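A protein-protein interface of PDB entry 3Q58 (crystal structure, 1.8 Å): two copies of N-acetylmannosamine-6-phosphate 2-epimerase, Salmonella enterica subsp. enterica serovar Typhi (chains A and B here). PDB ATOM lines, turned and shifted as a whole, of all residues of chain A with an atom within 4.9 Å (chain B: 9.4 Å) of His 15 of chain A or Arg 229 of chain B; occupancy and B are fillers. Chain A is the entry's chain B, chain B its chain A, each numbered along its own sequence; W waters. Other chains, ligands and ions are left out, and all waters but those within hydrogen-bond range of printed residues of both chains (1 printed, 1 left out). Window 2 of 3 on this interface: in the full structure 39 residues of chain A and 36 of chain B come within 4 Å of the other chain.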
ATOM      1  N   GLU A  11     -31.293 -37.172 -15.378  1.00  0.00           N
ATOM      2  CA  GLU A  11     -30.245 -37.470 -16.347  1.00  0.00           C
ATOM      3  C   GLU A  11     -30.792 -37.375 -17.769  1.00  0.00           C
ATOM      4  O   GLU A  11     -30.160 -36.798 -18.653  1.00  0.00           O
ATOM      5  CB  GLU A  11     -29.661 -38.862 -16.104  1.00  0.00           C
ATOM      6  CG  GLU A  11     -28.706 -38.935 -14.928  1.00  0.00           C
ATOM      7  CD  GLU A  11     -27.357 -38.316 -15.233  1.00  0.00           C
ATOM      8  OE1 GLU A  11     -27.168 -37.819 -16.362  1.00  0.00           O
ATOM      9  OE2 GLU A  11     -26.478 -38.331 -14.343  1.00  0.00           O
ATOM     10  N   GLN A  12     -31.969 -37.954 -17.983  1.00  0.00           N
ATOM     11  CA  GLN A  12     -32.600 -37.918 -19.298  1.00  0.00           C
ATOM     12  C   GLN A  12     -32.905 -36.479 -19.716  1.00  0.00           C
ATOM     13  O   GLN A  12     -32.569 -36.058 -20.824  1.00  0.00           O
ATOM     14  CB  GLN A  12     -33.870 -38.781 -19.319  1.00  0.00           C
ATOM     15  CG  GLN A  12     -33.601 -40.284 -19.256  1.00  0.00           C
ATOM     16  CD  GLN A  12     -34.873 -41.122 -19.217  1.00  0.00           C
ATOM     17  OE1 GLN A  12     -35.889 -40.708 -18.656  1.00  0.00           O
ATOM     18  NE2 GLN A  12     -34.819 -42.307 -19.817  1.00  0.00           N
ATOM     19  N   SER A  13     -33.523 -35.723 -18.816  1.00  0.00           N
ATOM     20  CA  SER A  13     -33.879 -34.331 -19.088  1.00  0.00           C
ATOM     21  C   SER A  13     -32.658 -33.454 -19.409  1.00  0.00           C
ATOM     22  O   SER A  13     -32.721 -32.587 -20.283  1.00  0.00           O
ATOM     23  CB  SER A  13     -34.649 -33.750 -17.900  1.00  0.00           C
ATOM     24  OG  SER A  13     -34.913 -32.375 -18.088  1.00  0.00           O
ATOM     25  N   VAL A  14     -31.554 -33.671 -18.697  1.00  0.00           N
ATOM     26  CA  VAL A  14     -30.312 -32.949 -18.969  1.00  0.00           C
ATOM     27  C   VAL A  14     -29.761 -33.282 -20.360  1.00  0.00           C
ATOM     28  O   VAL A  14     -29.336 -32.393 -21.096  1.00  0.00           O
ATOM     29  CB  VAL A  14     -29.233 -33.241 -17.895  1.00  0.00           C
ATOM     30  CG1 VAL A  14     -27.847 -32.859 -18.397  1.00  0.00           C
ATOM     31  CG2 VAL A  14     -29.556 -32.507 -16.606  1.00  0.00           C
ATOM     32  N   HIS A  15     -29.770 -34.561 -20.716  1.00  0.00           N
ATOM     33  CA  HIS A  15     -29.300 -34.985 -22.031  1.00  0.00           C
ATOM     34  C   HIS A  15     -30.131 -34.384 -23.174  1.00  0.00           C
ATOM     35  O   HIS A  15     -29.590 -33.973 -24.206  1.00  0.00           O
ATOM     36  CB  HIS A  15     -29.308 -36.512 -22.130  1.00  0.00           C
ATOM     37  CG  HIS A  15     -29.037 -37.029 -23.508  1.00  0.00           C
ATOM     38  ND1 HIS A  15     -30.044 -37.397 -24.377  1.00  0.00           N
ATOM     39  CD2 HIS A  15     -27.875 -37.236 -24.171  1.00  0.00           C
ATOM     40  CE1 HIS A  15     -29.513 -37.809 -25.512  1.00  0.00           C
ATOM     41  NE2 HIS A  15     -28.198 -37.724 -25.414  1.00  0.00           N
ATOM     42  N   GLU A  16     -31.446 -34.332 -22.982  1.00  0.00           N
ATOM     43  CA  GLU A  16     -32.360 -33.888 -24.031  1.00  0.00           C
ATOM     44  C   GLU A  16     -32.465 -32.368 -24.135  1.00  0.00           C
ATOM     45  O   GLU A  16     -32.623 -31.828 -25.229  1.00  0.00           O
ATOM     46  CB  GLU A  16     -33.752 -34.477 -23.797  1.00  0.00           C
ATOM     47  CG  GLU A  16     -33.771 -35.986 -23.680  1.00  0.00           C
ATOM     48  CD  GLU A  16     -35.109 -36.515 -23.199  1.00  0.00           C
ATOM     49  OE1 GLU A  16     -36.024 -35.696 -22.959  1.00  0.00           O
ATOM     50  OE2 GLU A  16     -35.242 -37.749 -23.057  1.00  0.00           O
ATOM     51  N   ASN A  17     -32.376 -31.683 -22.998  1.00  0.00           N
ATOM     52  CA  ASN A  17     -32.632 -30.241 -22.952  1.00  0.00           C
ATOM     53  C   ASN A  17     -31.380 -29.406 -22.721  1.00  0.00           C
ATOM     54  O   ASN A  17     -31.366 -28.206 -22.996  1.00  0.00           O
ATOM     55  CB  ASN A  17     -33.675 -29.911 -21.878  1.00  0.00           C
ATOM     56  CG  ASN A  17     -34.988 -30.638 -22.098  1.00  0.00           C
ATOM     57  OD1 ASN A  17     -35.679 -30.397 -23.083  1.00  0.00           O
ATOM     58  ND2 ASN A  17     -35.337 -31.533 -21.178  1.00  0.00           N
ATOM     59  N   GLY A  18     -30.327 -30.049 -22.227  1.00  0.00           N
ATOM     60  CA  GLY A  18     -29.144 -29.331 -21.791  1.00  0.00           C
ATOM     61  C   GLY A  18     -29.235 -29.050 -20.301  1.00  0.00           C
ATOM     62  O   GLY A  18     -30.327 -28.848 -19.765  1.00  0.00           O
ATOM     63  N   ILE A 200     -19.779 -26.202 -19.081  1.00  0.00           N
ATOM     64  CA  ILE A 200     -20.061 -27.491 -19.706  1.00  0.00           C
ATOM     65  C   ILE A 200     -18.797 -28.028 -20.376  1.00  0.00           C
ATOM     66  O   ILE A 200     -18.453 -29.204 -20.231  1.00  0.00           O
ATOM     67  CB  ILE A 200     -21.202 -27.375 -20.737  1.00  0.00           C
ATOM     68  CG1 ILE A 200     -22.495 -26.893 -20.059  1.00  0.00           C
ATOM     69  CG2 ILE A 200     -21.415 -28.696 -21.455  1.00  0.00           C
ATOM     70  CD1 ILE A 200     -23.057 -27.864 -19.025  1.00  0.00           C
ATOM     71  N   PHE B 223     -29.544 -19.256 -22.141  1.00  0.00           N
ATOM     72  CA  PHE B 223     -28.671 -20.126 -21.367  1.00  0.00           C
ATOM     73  C   PHE B 223     -28.847 -21.589 -21.768  1.00  0.00           C
ATOM     74  O   PHE B 223     -27.870 -22.322 -21.898  1.00  0.00           O
ATOM     75  CB  PHE B 223     -28.905 -19.930 -19.856  1.00  0.00           C
ATOM     76  CG  PHE B 223     -28.262 -18.683 -19.297  1.00  0.00           C
ATOM     77  CD1 PHE B 223     -26.977 -18.725 -18.769  1.00  0.00           C
ATOM     78  CD2 PHE B 223     -28.938 -17.472 -19.307  1.00  0.00           C
ATOM     79  CE1 PHE B 223     -26.381 -17.586 -18.260  1.00  0.00           C
ATOM     80  CE2 PHE B 223     -28.352 -16.324 -18.804  1.00  0.00           C
ATOM     81  CZ  PHE B 223     -27.070 -16.375 -18.277  1.00  0.00           C
ATOM     82  N   SER B 224     -30.056 -22.024 -21.975  1.00  0.00           N
ATOM     83  CA  SER B 224     -30.320 -23.390 -22.350  1.00  0.00           C
ATOM     84  C   SER B 224     -29.641 -23.706 -23.654  1.00  0.00           C
ATOM     85  O   SER B 224     -28.958 -24.669 -23.790  1.00  0.00           O
ATOM     86  CB  SER B 224     -31.801 -23.589 -22.447  1.00  0.00           C
ATOM     87  OG  SER B 224     -32.123 -24.786 -23.033  1.00  0.00           O
ATOM     88  N   HIS B 225     -29.718 -22.816 -24.587  1.00  0.00           N
ATOM     89  CA  HIS B 225     -29.039 -23.031 -25.800  1.00  0.00           C
ATOM     90  C   HIS B 225     -27.533 -23.155 -25.632  1.00  0.00           C
ATOM     91  O   HIS B 225     -26.926 -23.935 -26.291  1.00  0.00           O
ATOM     92  CB  HIS B 225     -29.331 -21.874 -26.706  1.00  0.00           C
ATOM     93  CG  HIS B 225     -28.639 -21.947 -28.006  1.00  0.00           C
ATOM     94  ND1 HIS B 225     -29.200 -22.539 -29.111  1.00  0.00           N
ATOM     95  CD2 HIS B 225     -27.436 -21.475 -28.399  1.00  0.00           C
ATOM     96  CE1 HIS B 225     -28.372 -22.426 -30.128  1.00  0.00           C
ATOM     97  NE2 HIS B 225     -27.296 -21.783 -29.720  1.00  0.00           N
ATOM     98  N   ALA B 226     -26.951 -22.348 -24.769  1.00  0.00           N
ATOM     99  CA  ALA B 226     -25.505 -22.356 -24.517  1.00  0.00           C
ATOM    100  C   ALA B 226     -24.992 -23.684 -23.917  1.00  0.00           C
ATOM    101  O   ALA B 226     -23.937 -24.120 -24.230  1.00  0.00           O
ATOM    102  CB  ALA B 226     -25.147 -21.263 -23.635  1.00  0.00           C
ATOM    103  N   VAL B 227     -25.753 -24.245 -23.016  1.00  0.00           N
ATOM    104  CA  VAL B 227     -25.353 -25.473 -22.328  1.00  0.00           C
ATOM    105  C   VAL B 227     -25.629 -26.780 -23.077  1.00  0.00           C
ATOM    106  O   VAL B 227     -25.122 -27.797 -22.720  1.00  0.00           O
ATOM    107  CB  VAL B 227     -25.925 -25.532 -20.947  1.00  0.00           C
ATOM    108  CG1 VAL B 227     -25.479 -24.381 -20.153  1.00  0.00           C
ATOM    109  CG2 VAL B 227     -27.340 -25.625 -20.958  1.00  0.00           C
ATOM    110  N   LYS B 228     -26.389 -26.759 -24.150  1.00  0.00           N
ATOM    111  CA  LYS B 228     -26.632 -28.023 -24.804  1.00  0.00           C
ATOM    112  C   LYS B 228     -25.355 -28.240 -25.532  1.00  0.00           C
ATOM    113  O   LYS B 228     -25.093 -27.650 -26.510  1.00  0.00           O
ATOM    114  CB  LYS B 228     -27.787 -27.942 -25.770  1.00  0.00           C
ATOM    115  CG  LYS B 228     -29.157 -27.829 -25.123  1.00  0.00           C
ATOM    116  CD  LYS B 228     -30.217 -28.569 -25.945  1.00  0.00           C
ATOM    117  CE  LYS B 228     -29.632 -29.851 -26.474  1.00  0.00           C
ATOM    118  NZ  LYS B 228     -30.492 -30.704 -27.303  1.00  0.00           N
ATOM    119  N   ARG B 229     -24.531 -29.104 -24.984  1.00  0.00           N
ATOM    120  CA  ARG B 229     -23.206 -29.393 -25.530  1.00  0.00           C
ATOM    121  C   ARG B 229     -22.361 -28.128 -25.697  1.00  0.00           C
ATOM    122  O   ARG B 229     -22.753 -27.032 -25.294  1.00  0.00           O
ATOM    123  CB  ARG B 229     -23.310 -30.151 -26.857  1.00  0.00           C
ATOM    124  CG  ARG B 229     -23.241 -31.666 -26.724  1.00  0.00           C
ATOM    125  CD  ARG B 229     -24.426 -32.231 -25.953  1.00  0.00           C
ATOM    126  NE  ARG B 229     -25.694 -31.983 -26.634  1.00  0.00           N
ATOM    127  CZ  ARG B 229     -26.846 -32.551 -26.296  1.00  0.00           C
ATOM    128  NH1 ARG B 229     -26.895 -33.412 -25.289  1.00  0.00           N
ATOM    129  NH2 ARG B 229     -27.952 -32.265 -26.971  1.00  0.00           N
ATOM    130  OXT ARG B 229     -21.254 -28.172 -26.235  1.00  0.00           O
HETATM  131  O   HOH W   1     -26.947 -31.764 -23.037  1.00  0.00           O
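O of Asn 17 of chain A touches OG of Ser 224 of chain B, 3.5 Å away.
Lys 228 of chain B touches Asn 17 of chain A.
C of Gly 18 of chain A touches CG2 of Val 227 of chain B, 3.97 Å away.
Gly 18 of chain A touches Lys 228 of chain B.
Ile 200 of chain A touches Val 227 of chain B (CG1 to CB, 3.8 Å).
Of chain B, only Arg 229 comes within 4 Å of His 15 of chain A.
Of chain A, only His 15 (3.0 Å) comes within 4 Å of Arg 229 of chain B.
No residue of chain B comes within 4 Å of Val 14 of chain A.
Of the printed residues of chain B, Glu 16 of chain A touches Lys 228 (3.2 Å).
Of the printed residues of chain B, Asn 17 of chain A touches Ser 224 and Lys 228.
Printed residues of chain A within 4 Å of Lys 228 of chain B: Glu 16 (3.2 Å), Asn 17 (3.1 Å) and Gly 18 (3.7 Å).
Printed residues of chain A within 4 Å of Ser 224 of chain B: Asn 17 (3.5 Å).
Of the printed residues of chain A, Val 227 of chain B touches Gly 18 and Ile 200.
Ala 226 of chain B touches none of the printed residues of chain A.
The nearest residue of chain A that does not touch Arg 229 of chain B is Ile 200 of chain A (4.4 Å).
The nearest printed residue of chain B that does not touch Glu 16 of chain A is Arg 229 of chain B (5.0 Å).
O of Glu 16 of chain A lies within hydrogen-bond range of NZ of Lys 228 of chain B (3.2 Å).
The guanidinium group (NH1) of Arg 229 of chain B lies within hydrogen-bond range of the backbone carbonyl oxygen (O) of His 15 of chain A (3.0 Å).
Water W1 lies within hydrogen-bond range of the guanidinium group of Arg 229 of chain B (2.8 Å) and the backbone carbonyl oxygen of Val 14 of chain A (3.1 Å).
No position is printed for both chains.
Of the 7 pairs that touch across the chains among the printed residues, none has its exchanged pair printed and touching as well.
Hydrophobic or aromatic side chains of chain A within 4 Å of the printed part of chain B: Ile 200.
Of the 7 printed residues of chain B, 4 touch a printed residue of chain A.
Hydrophobic or aromatic side chains of chain B that line the printed part of chain A: Val 227.
Along chain B the printed residues that touch a printed residue of chain A span positions 224 to 229.
The backbone carbonyl oxygen (O) of Ser 13 of chain A sits at hydrogen-bond distance from the side-chain amide nitrogen (ND2) of Asn 17 of chain A, at 3.0 Å.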
